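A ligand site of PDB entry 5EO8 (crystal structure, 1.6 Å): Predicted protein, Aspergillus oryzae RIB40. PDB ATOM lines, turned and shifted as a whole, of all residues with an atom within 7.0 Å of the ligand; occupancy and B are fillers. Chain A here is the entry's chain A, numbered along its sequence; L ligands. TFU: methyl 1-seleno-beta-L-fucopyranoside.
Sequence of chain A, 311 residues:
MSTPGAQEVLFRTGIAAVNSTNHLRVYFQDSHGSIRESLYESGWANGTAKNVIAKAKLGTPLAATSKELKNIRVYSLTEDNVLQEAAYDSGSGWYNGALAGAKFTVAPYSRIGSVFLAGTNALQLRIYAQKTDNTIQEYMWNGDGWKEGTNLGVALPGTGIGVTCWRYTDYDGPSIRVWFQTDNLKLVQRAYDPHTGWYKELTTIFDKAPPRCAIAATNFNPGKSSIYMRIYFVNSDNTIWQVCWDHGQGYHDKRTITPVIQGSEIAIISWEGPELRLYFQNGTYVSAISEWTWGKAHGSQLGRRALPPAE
An oxygen (O4) of the ligand sits at hydrogen-bond distance from the side-chain carboxylate (OE2) of Glu 291 (2.6 Å). The guanidinium group (NE) of Arg 277 lies within hydrogen-bond range of an oxygen (O4) of the ligand, 2.8 Å away. NE1 of Trp 44 lies within hydrogen-bond range of O3 of the ligand (2.8 Å).
The side-chain carboxylate of Glu 291 sits at hydrogen-bond distance from the backbone NH of Arg 304, 2.9 Å away. The side-chain carboxylate of Glu 291 lies within hydrogen-bond range of the side-chain hydroxyl of Tyr 279, 2.8 Å away. The backbone NH (N) of Gly 303 lies within hydrogen-bond range of the backbone carbonyl oxygen (O) of Glu 291, at 2.7 Å. The side-chain carboxylate of Glu 275 is in salt-bridge range of the guanidinium group of Arg 277 (2.9 Å). O of Arg 277 sits at hydrogen-bond distance from N of Ile 269, at 2.9 Å. The backbone carbonyl oxygen (O) of Leu 24 lies within hydrogen-bond range of the backbone NH (N) of Tyr 40 (2.8 Å).
Asn 22 touches the ligand. Leu 24 touches the ligand. Tyr 40 touches the ligand. CH2 of Trp 271 touches C6 of the ligand, at 3.9 Å. Arg 304 touches the ligand. Of the 22 residues printed, 8 come within 4 Å of the ligand.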
ATOM      1  N   THR A  21      26.704 -23.688  -9.130  1.00  0.00           N
ATOM      2  CA  THR A  21      26.789 -25.136  -9.308  1.00  0.00           C
ATOM      3  C   THR A  21      25.815 -25.582 -10.412  1.00  0.00           C
ATOM      4  O   THR A  21      25.929 -25.086 -11.539  1.00  0.00           O
ATOM      5  CB  THR A  21      26.540 -25.911  -7.973  1.00  0.00           C
ATOM      6  OG1 THR A  21      25.289 -25.539  -7.399  1.00  0.00           O
ATOM      7  CG2 THR A  21      27.660 -25.598  -6.984  1.00  0.00           C
ATOM      8  N   ASN A  22      24.876 -26.477 -10.131  1.00  0.00           N
ATOM      9  CA  ASN A  22      23.984 -27.000 -11.169  1.00  0.00           C
ATOM     10  C   ASN A  22      22.682 -26.208 -11.311  1.00  0.00           C
ATOM     11  O   ASN A  22      21.673 -26.721 -11.800  1.00  0.00           O
ATOM     12  CB  ASN A  22      23.676 -28.476 -10.902  1.00  0.00           C
ATOM     13  CG  ASN A  22      22.894 -28.702  -9.628  1.00  0.00           C
ATOM     14  OD1 ASN A  22      22.834 -27.828  -8.757  1.00  0.00           O
ATOM     15  ND2 ASN A  22      22.295 -29.876  -9.497  1.00  0.00           N
ATOM     16  N   HIS A  23      22.722 -24.943 -10.882  1.00  0.00           N
ATOM     17  CA  HIS A  23      21.653 -23.997 -11.150  1.00  0.00           C
ATOM     18  C   HIS A  23      22.087 -23.114 -12.311  1.00  0.00           C
ATOM     19  O   HIS A  23      23.013 -22.316 -12.174  1.00  0.00           O
ATOM     20  CB  HIS A  23      21.343 -23.146  -9.910  1.00  0.00           C
ATOM     21  CG  HIS A  23      21.077 -23.963  -8.674  1.00  0.00           C
ATOM     22  ND1 HIS A  23      19.811 -24.216  -8.212  1.00  0.00           N
ATOM     23  CD2 HIS A  23      21.924 -24.579  -7.816  1.00  0.00           C
ATOM     24  CE1 HIS A  23      19.879 -24.951  -7.112  1.00  0.00           C
ATOM     25  NE2 HIS A  23      21.154 -25.190  -6.857  1.00  0.00           N
ATOM     26  N   LEU A  24      21.440 -23.273 -13.471  1.00  0.00           N
ATOM     27  CA  LEU A  24      21.962 -22.727 -14.721  1.00  0.00           C
ATOM     28  C   LEU A  24      21.070 -21.654 -15.352  1.00  0.00           C
ATOM     29  O   LEU A  24      19.854 -21.680 -15.223  1.00  0.00           O
ATOM     30  CB  LEU A  24      22.142 -23.856 -15.743  1.00  0.00           C
ATOM     31  CG  LEU A  24      22.596 -25.215 -15.203  1.00  0.00           C
ATOM     32  CD1 LEU A  24      22.621 -26.233 -16.336  1.00  0.00           C
ATOM     33  CD2 LEU A  24      23.949 -25.117 -14.529  1.00  0.00           C
ATOM     34  N   TYR A  40      17.795 -23.544 -15.795  1.00  0.00           N
ATOM     35  CA  TYR A  40      17.710 -24.893 -15.263  1.00  0.00           C
ATOM     36  C   TYR A  40      17.673 -24.834 -13.751  1.00  0.00           C
ATOM     37  O   TYR A  40      18.643 -24.419 -13.106  1.00  0.00           O
ATOM     38  CB  TYR A  40      18.891 -25.754 -15.712  1.00  0.00           C
ATOM     39  CG  TYR A  40      18.785 -27.179 -15.243  1.00  0.00           C
ATOM     40  CD1 TYR A  40      18.119 -28.130 -16.008  1.00  0.00           C
ATOM     41  CD2 TYR A  40      19.321 -27.577 -14.023  1.00  0.00           C
ATOM     42  CE1 TYR A  40      18.000 -29.444 -15.572  1.00  0.00           C
ATOM     43  CE2 TYR A  40      19.206 -28.882 -13.590  1.00  0.00           C
ATOM     44  CZ  TYR A  40      18.552 -29.807 -14.362  1.00  0.00           C
ATOM     45  OH  TYR A  40      18.438 -31.113 -13.928  1.00  0.00           O
ATOM     46  N   GLY A  43      15.437 -28.897 -13.691  1.00  0.00           N
ATOM     47  CA  GLY A  43      14.607 -28.976 -14.870  1.00  0.00           C
ATOM     48  C   GLY A  43      14.677 -27.696 -15.689  1.00  0.00           C
ATOM     49  O   GLY A  43      14.836 -26.613 -15.139  1.00  0.00           O
ATOM     50  N   TRP A  44      14.564 -27.838 -17.006  1.00  0.00           N
ATOM     51  CA  TRP A  44      14.666 -26.712 -17.919  1.00  0.00           C
ATOM     52  C   TRP A  44      13.343 -25.975 -18.092  1.00  0.00           C
ATOM     53  O   TRP A  44      12.276 -26.596 -18.109  1.00  0.00           O
ATOM     54  CB  TRP A  44      15.163 -27.185 -19.288  1.00  0.00           C
ATOM     55  CG  TRP A  44      16.628 -27.494 -19.303  1.00  0.00           C
ATOM     56  CD1 TRP A  44      17.213 -28.732 -19.227  1.00  0.00           C
ATOM     57  CD2 TRP A  44      17.703 -26.557 -19.407  1.00  0.00           C
ATOM     58  NE1 TRP A  44      18.581 -28.608 -19.276  1.00  0.00           N
ATOM     59  CE2 TRP A  44      18.902 -27.289 -19.387  1.00  0.00           C
ATOM     60  CE3 TRP A  44      17.759 -25.162 -19.522  1.00  0.00           C
ATOM     61  CZ2 TRP A  44      20.152 -26.679 -19.476  1.00  0.00           C
ATOM     62  CZ3 TRP A  44      18.994 -24.550 -19.592  1.00  0.00           C
ATOM     63  CH2 TRP A  44      20.176 -25.309 -19.574  1.00  0.00           C
ATOM     64  N   ILE A 269      30.124 -23.526 -19.241  1.00  0.00           N
ATOM     65  CA  ILE A 269      30.117 -23.283 -17.797  1.00  0.00           C
ATOM     66  C   ILE A 269      30.654 -24.512 -17.094  1.00  0.00           C
ATOM     67  O   ILE A 269      30.732 -25.597 -17.664  1.00  0.00           O
ATOM     68  CB  ILE A 269      28.713 -22.962 -17.249  1.00  0.00           C
ATOM     69  CG1 ILE A 269      27.698 -24.003 -17.729  1.00  0.00           C
ATOM     70  CG2 ILE A 269      28.302 -21.564 -17.656  1.00  0.00           C
ATOM     71  CD1 ILE A 269      26.336 -23.870 -17.090  1.00  0.00           C
ATOM     72  N   TRP A 271      31.411 -26.313 -12.814  1.00  0.00           N
ATOM     73  CA  TRP A 271      31.476 -26.204 -11.363  1.00  0.00           C
ATOM     74  C   TRP A 271      32.245 -27.403 -10.822  1.00  0.00           C
ATOM     75  O   TRP A 271      32.542 -28.358 -11.544  1.00  0.00           O
ATOM     76  CB  TRP A 271      30.073 -26.103 -10.748  1.00  0.00           C
ATOM     77  CG  TRP A 271      29.104 -27.214 -11.024  1.00  0.00           C
ATOM     78  CD1 TRP A 271      28.789 -28.264 -10.194  1.00  0.00           C
ATOM     79  CD2 TRP A 271      28.294 -27.377 -12.186  1.00  0.00           C
ATOM     80  NE1 TRP A 271      27.848 -29.061 -10.775  1.00  0.00           N
ATOM     81  CE2 TRP A 271      27.520 -28.548 -12.009  1.00  0.00           C
ATOM     82  CE3 TRP A 271      28.143 -26.651 -13.380  1.00  0.00           C
ATOM     83  CZ2 TRP A 271      26.617 -28.999 -12.969  1.00  0.00           C
ATOM     84  CZ3 TRP A 271      27.244 -27.110 -14.319  1.00  0.00           C
ATOM     85  CH2 TRP A 271      26.491 -28.270 -14.108  1.00  0.00           C
ATOM     86  N   GLU A 275      32.224 -30.589 -13.223  1.00  0.00           N
ATOM     87  CA  GLU A 275      31.102 -30.732 -14.133  1.00  0.00           C
ATOM     88  C   GLU A 275      31.239 -29.679 -15.213  1.00  0.00           C
ATOM     89  O   GLU A 275      31.494 -28.510 -14.899  1.00  0.00           O
ATOM     90  CB  GLU A 275      29.765 -30.585 -13.397  1.00  0.00           C
ATOM     91  CG  GLU A 275      29.468 -31.701 -12.406  1.00  0.00           C
ATOM     92  CD  GLU A 275      29.002 -32.987 -13.057  1.00  0.00           C
ATOM     93  OE1 GLU A 275      28.389 -32.940 -14.155  1.00  0.00           O
ATOM     94  OE2 GLU A 275      29.253 -34.070 -12.473  1.00  0.00           O
ATOM     95  N   LEU A 276      31.093 -30.072 -16.467  1.00  0.00           N
ATOM     96  CA  LEU A 276      31.151 -29.156 -17.602  1.00  0.00           C
ATOM     97  C   LEU A 276      29.830 -29.172 -18.340  1.00  0.00           C
ATOM     98  O   LEU A 276      29.234 -30.241 -18.492  1.00  0.00           O
ATOM     99  CB  LEU A 276      32.269 -29.535 -18.567  1.00  0.00           C
ATOM    100  CG  LEU A 276      33.649 -29.786 -17.963  1.00  0.00           C
ATOM    101  CD1 LEU A 276      34.602 -30.249 -19.056  1.00  0.00           C
ATOM    102  CD2 LEU A 276      34.185 -28.549 -17.286  1.00  0.00           C
ATOM    103  N   ARG A 277      29.377 -28.005 -18.792  1.00  0.00           N
ATOM    104  CA  ARG A 277      28.230 -27.919 -19.693  1.00  0.00           C
ATOM    105  C   ARG A 277      28.542 -26.977 -20.846  1.00  0.00           C
ATOM    106  O   ARG A 277      28.906 -25.820 -20.637  1.00  0.00           O
ATOM    107  CB  ARG A 277      26.972 -27.436 -18.967  1.00  0.00           C
ATOM    108  CG  ARG A 277      26.551 -28.301 -17.801  1.00  0.00           C
ATOM    109  CD  ARG A 277      26.078 -29.686 -18.245  1.00  0.00           C
ATOM    110  NE  ARG A 277      25.562 -30.450 -17.118  1.00  0.00           N
ATOM    111  CZ  ARG A 277      26.302 -31.198 -16.303  1.00  0.00           C
ATOM    112  NH1 ARG A 277      27.615 -31.296 -16.469  1.00  0.00           N
ATOM    113  NH2 ARG A 277      25.724 -31.852 -15.297  1.00  0.00           N
ATOM    114  N   TYR A 279      27.153 -25.338 -24.541  1.00  0.00           N
ATOM    115  CA  TYR A 279      25.943 -25.002 -25.294  1.00  0.00           C
ATOM    116  C   TYR A 279      26.300 -24.494 -26.675  1.00  0.00           C
ATOM    117  O   TYR A 279      27.301 -23.818 -26.863  1.00  0.00           O
ATOM    118  CB  TYR A 279      25.103 -23.976 -24.526  1.00  0.00           C
ATOM    119  CG  TYR A 279      24.741 -24.512 -23.174  1.00  0.00           C
ATOM    120  CD1 TYR A 279      23.646 -25.355 -23.011  1.00  0.00           C
ATOM    121  CD2 TYR A 279      25.519 -24.222 -22.059  1.00  0.00           C
ATOM    122  CE1 TYR A 279      23.324 -25.871 -21.766  1.00  0.00           C
ATOM    123  CE2 TYR A 279      25.205 -24.734 -20.830  1.00  0.00           C
ATOM    124  CZ  TYR A 279      24.114 -25.552 -20.692  1.00  0.00           C
ATOM    125  OH  TYR A 279      23.804 -26.063 -19.453  1.00  0.00           O
ATOM    126  N   GLU A 291      22.900 -29.173 -25.595  1.00  0.00           N
ATOM    127  CA  GLU A 291      23.819 -29.219 -24.472  1.00  0.00           C
ATOM    128  C   GLU A 291      24.709 -30.457 -24.546  1.00  0.00           C
ATOM    129  O   GLU A 291      24.250 -31.543 -24.903  1.00  0.00           O
ATOM    130  CB  GLU A 291      23.026 -29.223 -23.150  1.00  0.00           C
ATOM    131  CG  GLU A 291      23.860 -29.328 -21.886  1.00  0.00           C
ATOM    132  CD  GLU A 291      22.992 -29.539 -20.661  1.00  0.00           C
ATOM    133  OE1 GLU A 291      22.271 -30.565 -20.615  1.00  0.00           O
ATOM    134  OE2 GLU A 291      23.014 -28.689 -19.739  1.00  0.00           O
ATOM    135  N   TRP A 292      25.990 -30.263 -24.230  1.00  0.00           N
ATOM    136  CA  TRP A 292      26.924 -31.370 -24.034  1.00  0.00           C
ATOM    137  C   TRP A 292      27.381 -31.306 -22.584  1.00  0.00           C
ATOM    138  O   TRP A 292      27.519 -30.222 -22.025  1.00  0.00           O
ATOM    139  CB  TRP A 292      28.112 -31.262 -25.003  1.00  0.00           C
ATOM    140  CG  TRP A 292      29.242 -32.232 -24.762  1.00  0.00           C
ATOM    141  CD1 TRP A 292      29.389 -33.468 -25.311  1.00  0.00           C
ATOM    142  CD2 TRP A 292      30.397 -32.013 -23.937  1.00  0.00           C
ATOM    143  NE1 TRP A 292      30.563 -34.041 -24.869  1.00  0.00           N
ATOM    144  CE2 TRP A 292      31.193 -33.166 -24.028  1.00  0.00           C
ATOM    145  CE3 TRP A 292      30.819 -30.960 -23.132  1.00  0.00           C
ATOM    146  CZ2 TRP A 292      32.395 -33.300 -23.338  1.00  0.00           C
ATOM    147  CZ3 TRP A 292      32.020 -31.094 -22.441  1.00  0.00           C
ATOM    148  CH2 TRP A 292      32.796 -32.245 -22.556  1.00  0.00           C
ATOM    149  N   THR A 293      27.583 -32.473 -21.973  1.00  0.00           N
ATOM    150  CA  THR A 293      27.916 -32.554 -20.557  1.00  0.00           C
ATOM    151  C   THR A 293      29.173 -33.373 -20.338  1.00  0.00           C
ATOM    152  O   THR A 293      29.487 -34.283 -21.114  1.00  0.00           O
ATOM    153  CB  THR A 293      26.766 -33.172 -19.732  1.00  0.00           C
ATOM    154  OG1 THR A 293      26.753 -34.598 -19.910  1.00  0.00           O
ATOM    155  CG2 THR A 293      25.417 -32.601 -20.148  1.00  0.00           C
ATOM    156  N   HIS A 298      29.841 -40.254 -15.823  1.00  0.00           N
ATOM    157  CA  HIS A 298      29.546 -40.782 -17.156  1.00  0.00           C
ATOM    158  C   HIS A 298      30.437 -40.197 -18.258  1.00  0.00           C
ATOM    159  O   HIS A 298      30.288 -40.554 -19.425  1.00  0.00           O
ATOM    160  CB  HIS A 298      28.079 -40.542 -17.489  1.00  0.00           C
ATOM    161  CG  HIS A 298      27.130 -41.128 -16.493  1.00  0.00           C
ATOM    162  ND1 HIS A 298      26.919 -42.488 -16.386  1.00  0.00           N
ATOM    163  CD2 HIS A 298      26.351 -40.549 -15.552  1.00  0.00           C
ATOM    164  CE1 HIS A 298      26.036 -42.718 -15.430  1.00  0.00           C
ATOM    165  NE2 HIS A 298      25.672 -41.559 -14.909  1.00  0.00           N
ATOM    166  N   GLN A 301      29.007 -36.919 -22.510  1.00  0.00           N
ATOM    167  CA  GLN A 301      27.664 -37.318 -22.896  1.00  0.00           C
ATOM    168  C   GLN A 301      26.875 -36.102 -23.363  1.00  0.00           C
ATOM    169  O   GLN A 301      26.989 -35.018 -22.803  1.00  0.00           O
ATOM    170  CB  GLN A 301      26.940 -37.999 -21.734  1.00  0.00           C
ATOM    171  CG  GLN A 301      25.588 -38.586 -22.118  1.00  0.00           C
ATOM    172  CD  GLN A 301      24.857 -39.253 -20.963  1.00  0.00           C
ATOM    173  OE1 GLN A 301      25.441 -39.476 -19.897  1.00  0.00           O
ATOM    174  NE2 GLN A 301      23.589 -39.571 -21.169  1.00  0.00           N
ATOM    175  N   LEU A 302      26.070 -36.280 -24.405  1.00  0.00           N
ATOM    176  CA  LEU A 302      25.163 -35.230 -24.808  1.00  0.00           C
ATOM    177  C   LEU A 302      24.136 -35.027 -23.710  1.00  0.00           C
ATOM    178  O   LEU A 302      23.714 -35.983 -23.056  1.00  0.00           O
ATOM    179  CB  LEU A 302      24.490 -35.560 -26.144  1.00  0.00           C
ATOM    180  CG  LEU A 302      25.354 -35.327 -27.379  1.00  0.00           C
ATOM    181  CD1 LEU A 302      24.673 -35.889 -28.621  1.00  0.00           C
ATOM    182  CD2 LEU A 302      25.642 -33.834 -27.572  1.00  0.00           C
ATOM    183  N   GLY A 303      23.745 -33.777 -23.490  1.00  0.00           N
ATOM    184  CA  GLY A 303      22.754 -33.444 -22.482  1.00  0.00           C
ATOM    185  C   GLY A 303      21.415 -33.127 -23.109  1.00  0.00           C
ATOM    186  O   GLY A 303      20.981 -33.780 -24.052  1.00  0.00           O
ATOM    187  N   ARG A 304      20.761 -32.109 -22.558  1.00  0.00           N
ATOM    188  CA  ARG A 304      19.496 -31.616 -23.074  1.00  0.00           C
ATOM    189  C   ARG A 304      19.578 -31.402 -24.589  1.00  0.00           C
ATOM    190  O   ARG A 304      20.397 -30.616 -25.063  1.00  0.00           O
ATOM    191  CB  ARG A 304      19.114 -30.307 -22.366  1.00  0.00           C
ATOM    192  CG  ARG A 304      17.858 -29.634 -22.875  1.00  0.00           C
ATOM    193  CD  ARG A 304      16.582 -30.332 -22.439  1.00  0.00           C
ATOM    194  NE  ARG A 304      15.424 -29.593 -22.952  1.00  0.00           N
ATOM    195  CZ  ARG A 304      14.254 -29.475 -22.334  1.00  0.00           C
ATOM    196  NH1 ARG A 304      14.029 -30.044 -21.165  1.00  0.00           N
ATOM    197  NH2 ARG A 304      13.288 -28.761 -22.912  1.00  0.00           N
ATOM    198  N   LEU A 307      17.045 -27.057 -25.796  1.00  0.00           N
ATOM    199  CA  LEU A 307      16.738 -26.165 -24.692  1.00  0.00           C
ATOM    200  C   LEU A 307      15.420 -25.445 -24.921  1.00  0.00           C
ATOM    201  O   LEU A 307      15.019 -25.227 -26.071  1.00  0.00           O
ATOM    202  CB  LEU A 307      17.857 -25.135 -24.502  1.00  0.00           C
ATOM    203  CG  LEU A 307      18.963 -25.457 -23.492  1.00  0.00           C
ATOM    204  CD1 LEU A 307      19.866 -26.584 -23.976  1.00  0.00           C
ATOM    205  CD2 LEU A 307      19.769 -24.194 -23.227  1.00  0.00           C
HETATM  206  C1  TFU L   1      21.972 -32.811 -16.014  1.00  0.00           C
HETATM  207  C2  TFU L   1      21.533 -32.406 -17.421  1.00  0.00           C
HETATM  208  O2  TFU L   1      20.685 -33.421 -17.979  1.00  0.00           O
HETATM  209  C3  TFU L   1      20.798 -31.076 -17.368  1.00  0.00           C
HETATM  210  O3  TFU L   1      20.515 -30.594 -18.686  1.00  0.00           O
HETATM  211  C4  TFU L   1      21.656 -30.050 -16.629  1.00  0.00           C
HETATM  212  O4  TFU L   1      22.831 -29.792 -17.401  1.00  0.00           O
HETATM  213  C5  TFU L   1      22.042 -30.587 -15.256  1.00  0.00           C
HETATM  214  C6  TFU L   1      22.839 -29.571 -14.444  1.00  0.00           C
HETATM  215  O5  TFU L   1      22.796 -31.782 -15.447  1.00  0.00           O
HETATM  216 SE1  TFU L   1      22.947 -34.498 -16.091  1.00  0.00          SE
HETATM  217  C7  TFU L   1      21.389 -35.655 -15.952  1.00  0.00           C
